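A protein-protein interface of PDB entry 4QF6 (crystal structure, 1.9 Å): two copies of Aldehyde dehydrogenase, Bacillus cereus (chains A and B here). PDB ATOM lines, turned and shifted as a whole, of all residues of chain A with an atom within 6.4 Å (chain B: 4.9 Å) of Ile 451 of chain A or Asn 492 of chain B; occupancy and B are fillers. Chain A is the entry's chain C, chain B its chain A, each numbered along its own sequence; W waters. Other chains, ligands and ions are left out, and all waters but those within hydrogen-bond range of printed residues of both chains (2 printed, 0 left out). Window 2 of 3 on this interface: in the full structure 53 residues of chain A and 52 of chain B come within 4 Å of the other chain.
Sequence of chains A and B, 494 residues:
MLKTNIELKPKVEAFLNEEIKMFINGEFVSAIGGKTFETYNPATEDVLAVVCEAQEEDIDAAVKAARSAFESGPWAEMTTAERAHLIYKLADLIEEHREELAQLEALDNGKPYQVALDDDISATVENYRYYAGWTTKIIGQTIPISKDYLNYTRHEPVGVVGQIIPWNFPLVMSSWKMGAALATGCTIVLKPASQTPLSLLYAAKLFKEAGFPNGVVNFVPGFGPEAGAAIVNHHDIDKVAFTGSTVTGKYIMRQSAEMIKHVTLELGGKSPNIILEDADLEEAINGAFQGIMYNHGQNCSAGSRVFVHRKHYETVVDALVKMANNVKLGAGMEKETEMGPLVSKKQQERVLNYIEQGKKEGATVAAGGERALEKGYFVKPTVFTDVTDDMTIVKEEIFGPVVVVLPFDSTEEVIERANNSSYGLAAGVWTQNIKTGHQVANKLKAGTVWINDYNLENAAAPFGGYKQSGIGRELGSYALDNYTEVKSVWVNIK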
ATOM      1  N   ALA A 427      18.387  24.711  12.668  1.00  0.00           N
ATOM      2  CA  ALA A 427      16.984  24.832  12.277  1.00  0.00           C
ATOM      3  C   ALA A 427      16.784  24.172  10.938  1.00  0.00           C
ATOM      4  O   ALA A 427      17.648  24.173  10.115  1.00  0.00           O
ATOM      5  CB  ALA A 427      16.577  26.294  12.119  1.00  0.00           C
ATOM      6  N   GLY A 428      15.578  23.648  10.750  1.00  0.00           N
ATOM      7  CA  GLY A 428      15.092  23.167   9.495  1.00  0.00           C
ATOM      8  C   GLY A 428      13.842  23.904   9.039  1.00  0.00           C
ATOM      9  O   GLY A 428      13.010  24.337   9.837  1.00  0.00           O
ATOM     10  N   VAL A 429      13.764  24.069   7.733  1.00  0.00           N
ATOM     11  CA  VAL A 429      12.737  24.780   7.058  1.00  0.00           C
ATOM     12  C   VAL A 429      12.288  23.925   5.852  1.00  0.00           C
ATOM     13  O   VAL A 429      13.053  23.684   4.975  1.00  0.00           O
ATOM     14  CB  VAL A 429      13.260  26.125   6.485  1.00  0.00           C
ATOM     15  CG1 VAL A 429      12.081  26.878   5.872  1.00  0.00           C
ATOM     16  CG2 VAL A 429      13.892  26.945   7.593  1.00  0.00           C
ATOM     17  N   TRP A 430      11.035  23.554   5.798  1.00  0.00           N
ATOM     18  CA  TRP A 430      10.488  22.775   4.724  1.00  0.00           C
ATOM     19  C   TRP A 430       9.438  23.622   3.956  1.00  0.00           C
ATOM     20  O   TRP A 430       8.428  24.051   4.537  1.00  0.00           O
ATOM     21  CB  TRP A 430       9.852  21.473   5.298  1.00  0.00           C
ATOM     22  CG  TRP A 430      10.864  20.610   5.940  1.00  0.00           C
ATOM     23  CD1 TRP A 430      11.269  20.724   7.181  1.00  0.00           C
ATOM     24  CD2 TRP A 430      11.619  19.558   5.365  1.00  0.00           C
ATOM     25  NE1 TRP A 430      12.198  19.806   7.471  1.00  0.00           N
ATOM     26  CE2 TRP A 430      12.448  19.073   6.351  1.00  0.00           C
ATOM     27  CE3 TRP A 430      11.617  18.922   4.139  1.00  0.00           C
ATOM     28  CZ2 TRP A 430      13.282  17.978   6.164  1.00  0.00           C
ATOM     29  CZ3 TRP A 430      12.488  17.848   3.946  1.00  0.00           C
ATOM     30  CH2 TRP A 430      13.294  17.397   4.948  1.00  0.00           C
ATOM     31  N   THR A 431       9.729  23.930   2.682  1.00  0.00           N
ATOM     32  CA  THR A 431       8.878  24.735   1.823  1.00  0.00           C
ATOM     33  C   THR A 431       9.396  24.506   0.406  1.00  0.00           C
ATOM     34  O   THR A 431      10.625  24.463   0.166  1.00  0.00           O
ATOM     35  CB  THR A 431       8.905  26.289   2.122  1.00  0.00           C
ATOM     36  OG1 THR A 431       8.225  27.056   1.080  1.00  0.00           O
ATOM     37  CG2 THR A 431      10.351  26.846   2.307  1.00  0.00           C
ATOM     38  N   ASN A 433       8.865  26.714  -1.986  1.00  0.00           N
ATOM     39  CA  ASN A 433       8.971  28.028  -2.565  1.00  0.00           C
ATOM     40  C   ASN A 433      10.374  28.620  -2.413  1.00  0.00           C
ATOM     41  O   ASN A 433      10.902  28.778  -1.318  1.00  0.00           O
ATOM     42  CB  ASN A 433       7.927  28.997  -1.987  1.00  0.00           C
ATOM     43  CG  ASN A 433       7.810  30.251  -2.802  1.00  0.00           C
ATOM     44  OD1 ASN A 433       7.022  30.324  -3.779  1.00  0.00           O
ATOM     45  ND2 ASN A 433       8.696  31.187  -2.543  1.00  0.00           N
ATOM     46  N   GLY A 437      11.882  29.795   1.251  1.00  0.00           N
ATOM     47  CA  GLY A 437      13.006  29.014   1.870  1.00  0.00           C
ATOM     48  C   GLY A 437      14.189  29.919   2.299  1.00  0.00           C
ATOM     49  O   GLY A 437      14.653  29.892   3.422  1.00  0.00           O
ATOM     50  N   HIS A 438      14.653  30.732   1.390  1.00  0.00           N
ATOM     51  CA  HIS A 438      15.750  31.674   1.716  1.00  0.00           C
ATOM     52  C   HIS A 438      15.358  32.746   2.735  1.00  0.00           C
ATOM     53  O   HIS A 438      16.157  33.093   3.579  1.00  0.00           O
ATOM     54  CB  HIS A 438      16.362  32.283   0.429  1.00  0.00           C
ATOM     55  CG  HIS A 438      17.092  31.290  -0.398  1.00  0.00           C
ATOM     56  ND1 HIS A 438      16.604  30.839  -1.605  1.00  0.00           N
ATOM     57  CD2 HIS A 438      18.262  30.633  -0.209  1.00  0.00           C
ATOM     58  CE1 HIS A 438      17.432  29.969  -2.131  1.00  0.00           C
ATOM     59  NE2 HIS A 438      18.442  29.821  -1.307  1.00  0.00           N
ATOM     60  N   ALA A 441      15.142  30.994   6.212  1.00  0.00           N
ATOM     61  CA  ALA A 441      16.556  30.707   6.547  1.00  0.00           C
ATOM     62  C   ALA A 441      17.309  31.949   7.037  1.00  0.00           C
ATOM     63  O   ALA A 441      18.003  31.871   8.063  1.00  0.00           O
ATOM     64  CB  ALA A 441      17.286  30.072   5.438  1.00  0.00           C
ATOM     65  N   VAL A 449      21.227  26.013   9.059  1.00  0.00           N
ATOM     66  CA  VAL A 449      19.831  25.981   8.596  1.00  0.00           C
ATOM     67  C   VAL A 449      19.846  25.060   7.413  1.00  0.00           C
ATOM     68  O   VAL A 449      20.576  25.306   6.476  1.00  0.00           O
ATOM     69  CB  VAL A 449      19.277  27.361   8.173  1.00  0.00           C
ATOM     70  CG1 VAL A 449      17.830  27.232   7.658  1.00  0.00           C
ATOM     71  CG2 VAL A 449      19.262  28.345   9.325  1.00  0.00           C
ATOM     72  N   TRP A 450      19.033  23.979   7.486  1.00  0.00           N
ATOM     73  CA  TRP A 450      18.821  23.099   6.339  1.00  0.00           C
ATOM     74  C   TRP A 450      17.494  23.428   5.722  1.00  0.00           C
ATOM     75  O   TRP A 450      16.500  23.458   6.457  1.00  0.00           O
ATOM     76  CB  TRP A 450      18.742  21.648   6.833  1.00  0.00           C
ATOM     77  CG  TRP A 450      20.020  21.174   7.581  1.00  0.00           C
ATOM     78  CD1 TRP A 450      21.198  20.829   7.048  1.00  0.00           C
ATOM     79  CD2 TRP A 450      20.158  20.991   9.005  1.00  0.00           C
ATOM     80  NE1 TRP A 450      22.078  20.460   8.018  1.00  0.00           N
ATOM     81  CE2 TRP A 450      21.463  20.545   9.239  1.00  0.00           C
ATOM     82  CE3 TRP A 450      19.322  21.165  10.065  1.00  0.00           C
ATOM     83  CZ2 TRP A 450      21.928  20.263  10.488  1.00  0.00           C
ATOM     84  CZ3 TRP A 450      19.775  20.884  11.323  1.00  0.00           C
ATOM     85  CH2 TRP A 450      21.107  20.467  11.524  1.00  0.00           C
ATOM     86  N   ILE A 451      17.470  23.611   4.404  1.00  0.00           N
ATOM     87  CA  ILE A 451      16.268  23.884   3.646  1.00  0.00           C
ATOM     88  C   ILE A 451      15.864  22.639   2.914  1.00  0.00           C
ATOM     89  O   ILE A 451      16.489  22.188   2.001  1.00  0.00           O
ATOM     90  CB  ILE A 451      16.334  25.126   2.732  1.00  0.00           C
ATOM     91  CG1 ILE A 451      16.894  26.331   3.474  1.00  0.00           C
ATOM     92  CG2 ILE A 451      14.936  25.420   2.153  1.00  0.00           C
ATOM     93  CD1 ILE A 451      17.253  27.464   2.511  1.00  0.00           C
ATOM     94  N   ASN A 452      14.781  22.074   3.352  1.00  0.00           N
ATOM     95  CA  ASN A 452      14.319  20.821   2.857  1.00  0.00           C
ATOM     96  C   ASN A 452      15.205  19.585   3.190  1.00  0.00           C
ATOM     97  O   ASN A 452      15.410  18.725   2.341  1.00  0.00           O
ATOM     98  CB  ASN A 452      13.947  20.949   1.403  1.00  0.00           C
ATOM     99  CG  ASN A 452      12.771  21.893   1.195  1.00  0.00           C
ATOM    100  OD1 ASN A 452      11.759  21.876   1.951  1.00  0.00           O
ATOM    101  ND2 ASN A 452      12.870  22.698   0.183  1.00  0.00           N
ATOM    102  N   ASP A 453      15.769  19.576   4.389  1.00  0.00           N
ATOM    103  CA  ASP A 453      16.534  18.483   4.880  1.00  0.00           C
ATOM    104  C   ASP A 453      16.742  18.725   6.358  1.00  0.00           C
ATOM    105  O   ASP A 453      16.250  19.696   6.921  1.00  0.00           O
ATOM    106  CB  ASP A 453      17.857  18.300   4.094  1.00  0.00           C
ATOM    107  CG  ASP A 453      18.191  16.844   3.876  1.00  0.00           C
ATOM    108  OD1 ASP A 453      18.018  16.056   4.806  1.00  0.00           O
ATOM    109  OD2 ASP A 453      18.543  16.480   2.764  1.00  0.00           O
ATOM    110  N   TYR A 454      17.472  17.827   6.990  1.00  0.00           N
ATOM    111  CA  TYR A 454      17.759  18.010   8.421  1.00  0.00           C
ATOM    112  C   TYR A 454      18.942  17.128   8.802  1.00  0.00           C
ATOM    113  O   TYR A 454      19.130  16.103   8.180  1.00  0.00           O
ATOM    114  CB  TYR A 454      16.542  17.686   9.314  1.00  0.00           C
ATOM    115  CG  TYR A 454      16.620  18.408  10.642  1.00  0.00           C
ATOM    116  CD1 TYR A 454      17.308  17.876  11.725  1.00  0.00           C
ATOM    117  CD2 TYR A 454      16.145  19.708  10.770  1.00  0.00           C
ATOM    118  CE1 TYR A 454      17.423  18.569  12.936  1.00  0.00           C
ATOM    119  CE2 TYR A 454      16.317  20.427  11.962  1.00  0.00           C
ATOM    120  CZ  TYR A 454      16.929  19.833  13.039  1.00  0.00           C
ATOM    121  OH  TYR A 454      17.129  20.465  14.244  1.00  0.00           O
ATOM    122  N   LEU A 456      22.343  17.291   8.458  1.00  0.00           N
ATOM    123  CA  LEU A 456      23.485  17.066   7.573  1.00  0.00           C
ATOM    124  C   LEU A 456      24.672  17.800   8.120  1.00  0.00           C
ATOM    125  O   LEU A 456      24.535  18.986   8.444  1.00  0.00           O
ATOM    126  CB  LEU A 456      23.216  17.630   6.167  1.00  0.00           C
ATOM    127  CG  LEU A 456      21.922  17.076   5.579  1.00  0.00           C
ATOM    128  CD1 LEU A 456      21.798  17.609   4.150  1.00  0.00           C
ATOM    129  CD2 LEU A 456      21.789  15.559   5.665  1.00  0.00           C
ATOM    130  N   ASP B 148      24.164  17.200  -4.764  1.00  0.00           N
ATOM    131  CA  ASP B 148      22.851  17.173  -4.167  1.00  0.00           C
ATOM    132  C   ASP B 148      22.463  18.455  -3.384  1.00  0.00           C
ATOM    133  O   ASP B 148      21.294  18.567  -2.997  1.00  0.00           O
ATOM    134  CB  ASP B 148      22.702  15.994  -3.208  1.00  0.00           C
ATOM    135  CG  ASP B 148      22.763  14.582  -3.898  1.00  0.00           C
ATOM    136  OD1 ASP B 148      23.075  13.635  -3.206  1.00  0.00           O
ATOM    137  OD2 ASP B 148      22.603  14.490  -5.092  1.00  0.00           O
ATOM    138  N   TYR B 149      23.432  19.287  -2.987  1.00  0.00           N
ATOM    139  CA  TYR B 149      23.169  20.454  -2.133  1.00  0.00           C
ATOM    140  C   TYR B 149      23.875  21.698  -2.673  1.00  0.00           C
ATOM    141  O   TYR B 149      24.901  21.601  -3.256  1.00  0.00           O
ATOM    142  CB  TYR B 149      23.695  20.202  -0.682  1.00  0.00           C
ATOM    143  CG  TYR B 149      22.999  19.058  -0.073  1.00  0.00           C
ATOM    144  CD1 TYR B 149      21.770  19.226   0.470  1.00  0.00           C
ATOM    145  CD2 TYR B 149      23.520  17.779  -0.143  1.00  0.00           C
ATOM    146  CE1 TYR B 149      21.037  18.160   0.941  1.00  0.00           C
ATOM    147  CE2 TYR B 149      22.774  16.702   0.325  1.00  0.00           C
ATOM    148  CZ  TYR B 149      21.534  16.924   0.873  1.00  0.00           C
ATOM    149  OH  TYR B 149      20.761  15.862   1.389  1.00  0.00           O
ATOM    150  N   VAL B 489      24.136  27.347   5.509  1.00  0.00           N
ATOM    151  CA  VAL B 489      22.829  27.068   4.852  1.00  0.00           C
ATOM    152  C   VAL B 489      23.057  25.931   3.930  1.00  0.00           C
ATOM    153  O   VAL B 489      23.900  25.986   3.075  1.00  0.00           O
ATOM    154  CB  VAL B 489      22.228  28.283   4.073  1.00  0.00           C
ATOM    155  CG1 VAL B 489      20.827  27.922   3.502  1.00  0.00           C
ATOM    156  CG2 VAL B 489      22.001  29.492   4.986  1.00  0.00           C
ATOM    157  N   TRP B 490      22.237  24.911   4.064  1.00  0.00           N
ATOM    158  CA  TRP B 490      22.225  23.793   3.182  1.00  0.00           C
ATOM    159  C   TRP B 490      20.927  23.812   2.404  1.00  0.00           C
ATOM    160  O   TRP B 490      19.899  23.760   3.020  1.00  0.00           O
ATOM    161  CB  TRP B 490      22.221  22.509   3.997  1.00  0.00           C
ATOM    162  CG  TRP B 490      23.436  22.179   4.755  1.00  0.00           C
ATOM    163  CD1 TRP B 490      23.878  22.784   5.875  1.00  0.00           C
ATOM    164  CD2 TRP B 490      24.311  21.081   4.517  1.00  0.00           C
ATOM    165  NE1 TRP B 490      25.051  22.165   6.315  1.00  0.00           N
ATOM    166  CE2 TRP B 490      25.308  21.096   5.520  1.00  0.00           C
ATOM    167  CE3 TRP B 490      24.323  20.070   3.607  1.00  0.00           C
ATOM    168  CZ2 TRP B 490      26.334  20.111   5.602  1.00  0.00           C
ATOM    169  CZ3 TRP B 490      25.362  19.131   3.635  1.00  0.00           C
ATOM    170  CH2 TRP B 490      26.365  19.186   4.611  1.00  0.00           C
ATOM    171  N   VAL B 491      20.963  23.836   1.081  1.00  0.00           N
ATOM    172  CA  VAL B 491      19.776  23.776   0.230  1.00  0.00           C
ATOM    173  C   VAL B 491      19.696  22.448  -0.498  1.00  0.00           C
ATOM    174  O   VAL B 491      20.411  22.210  -1.423  1.00  0.00           O
ATOM    175  CB  VAL B 491      19.723  24.859  -0.867  1.00  0.00           C
ATOM    176  CG1 VAL B 491      18.318  24.880  -1.505  1.00  0.00           C
ATOM    177  CG2 VAL B 491      20.146  26.224  -0.341  1.00  0.00           C
ATOM    178  N   ASN B 492      18.784  21.573  -0.078  1.00  0.00           N
ATOM    179  CA  ASN B 492      18.576  20.323  -0.823  1.00  0.00           C
ATOM    180  C   ASN B 492      18.110  20.640  -2.220  1.00  0.00           C
ATOM    181  O   ASN B 492      17.109  21.320  -2.434  1.00  0.00           O
ATOM    182  CB  ASN B 492      17.588  19.424  -0.034  1.00  0.00           C
ATOM    183  CG  ASN B 492      17.412  18.018  -0.608  1.00  0.00           C
ATOM    184  OD1 ASN B 492      17.331  17.000   0.108  1.00  0.00           O
ATOM    185  ND2 ASN B 492      17.256  17.954  -1.851  1.00  0.00           N
ATOM    186  N   ILE B 493      18.871  20.170  -3.207  1.00  0.00           N
ATOM    187  CA  ILE B 493      18.513  20.361  -4.643  1.00  0.00           C
ATOM    188  C   ILE B 493      18.484  19.025  -5.404  1.00  0.00           C
ATOM    189  O   ILE B 493      18.668  18.964  -6.624  1.00  0.00           O
ATOM    190  CB  ILE B 493      19.420  21.372  -5.355  1.00  0.00           C
ATOM    191  CG1 ILE B 493      20.820  20.838  -5.455  1.00  0.00           C
ATOM    192  CG2 ILE B 493      19.294  22.729  -4.674  1.00  0.00           C
ATOM    193  CD1 ILE B 493      21.928  21.844  -5.642  1.00  0.00           C
ATOM    194  N   LYS B 494      18.238  17.951  -4.695  1.00  0.00           N
ATOM    195  CA  LYS B 494      18.193  16.612  -5.324  1.00  0.00           C
ATOM    196  C   LYS B 494      16.964  16.465  -6.191  1.00  0.00           C
ATOM    197  O   LYS B 494      15.947  17.057  -5.882  1.00  0.00           O
ATOM    198  CB  LYS B 494      18.073  15.494  -4.298  1.00  0.00           C
ATOM    199  CG  LYS B 494      19.237  15.231  -3.396  1.00  0.00           C
ATOM    200  CD  LYS B 494      19.016  13.960  -2.540  1.00  0.00           C
ATOM    201  CE  LYS B 494      19.858  14.038  -1.285  1.00  0.00           C
ATOM    202  NZ  LYS B 494      19.583  13.011  -0.277  1.00  0.00           N
ATOM    203  OXT LYS B 494      16.997  15.723  -7.177  1.00  0.00           O
HETATM  204  O   HOH W   1      13.900  17.570   0.396  1.00  0.00           O
HETATM  205  O   HOH W   2      15.710  22.880  -0.843  1.00  0.00           O
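OH of Tyr 149 of chain B is in hydrogen-bond range of OD2 of Asp 453 of chain A. The backbone NH of Asn 492 of chain B lies within hydrogen-bond range of the backbone carbonyl oxygen of Ile 451 of chain A, at 3.2 Å. The backbone carbonyl oxygen of Asn 452 of chain A lies close to the side-chain amide oxygen of Asn 492 of chain B, at 3.4 Å. O of Val 449 of chain A is in hydrogen-bond range of N of Trp 490 of chain B. OD2 of Asp 453 of chain A lies close to OD1 of Asn 492 of chain B (3.0 Å). O of Trp 490 of chain B sits at hydrogen-bond distance from N of Ile 451 of chain A (2.8 Å).
NE1 of Trp 450 of chain A sits at hydrogen-bond distance from O of Leu 456 of chain A, at 2.9 Å. O of Val 429 of chain A sits at hydrogen-bond distance from N of Asn 452 of chain A (2.9 Å). The backbone NH of Lys 494 of chain B lies close to the side-chain amide nitrogen of Asn 492 of chain B (3.0 Å). The backbone carbonyl oxygen of Thr 431 of chain A lies within hydrogen-bond range of the side-chain amide nitrogen of Asn 452 of chain A (2.9 Å). The backbone carbonyl oxygen (O) of Trp 450 of chain A lies within hydrogen-bond range of the backbone NH (N) of Val 429 of chain A. O of Ala 427 of chain A lies within hydrogen-bond range of N of Trp 450 of chain A (3.0 Å).
Val 449 of chain A touches Val 489 of chain B (O to CA, 3.3 Å). Trp 490 of chain B touches Trp 450 of chain A. Val 489 of chain B touches Ile 451 of chain A (CG1 to CD1, 3.7 Å). CD1 of Leu 456 of chain A touches CE1 of Tyr 149 of chain B, 3.3 Å away. O of Leu 456 of chain A touches CZ2 of Trp 490 of chain B (3.5 Å).
Ile 451 of chain A touches three residues of chain B. Of the printed residues of chain B, Asn 452 of chain A touches Asn 492 (3.3 Å). Printed residues of chain A within 4 Å of Val 489 of chain B: Val 449 and Ile 451. Printed residues of chain A within 4 Å of Trp 490 of chain B: Val 449, Trp 450, Ile 451 and Leu 456. The nearest residue of chain A that does not touch Asn 492 of chain B is Leu 456 of chain A (6.1 Å).
Hydrophobic or aromatic side chains of chain A within 4 Å of the printed part of chain B: Trp 450, Ile 451 and Leu 456. Of the 8 printed residues of chain B, 4 touch a printed residue of chain A. Hydrophobic or aromatic side chains of chain B that line the printed part of chain A: Tyr 149, Val 489 and Trp 490. Among the printed residues, no Asp or Glu carboxylate lies within 4 Å of a Lys or Arg side-chain nitrogen of the other chain.
No position is printed for both chains.
Water W2 lies within hydrogen-bond range of O of Asn 492 of chain B (2.6 Å), ND2 of Asn 452 of chain A (3.0 Å) and O of Ile 451 of chain A (3.0 Å). Water W1 lies within hydrogen-bond range of O of Asn 452 of chain A (2.7 Å) and OD1 of Asn 492 of chain B (3.5 Å).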
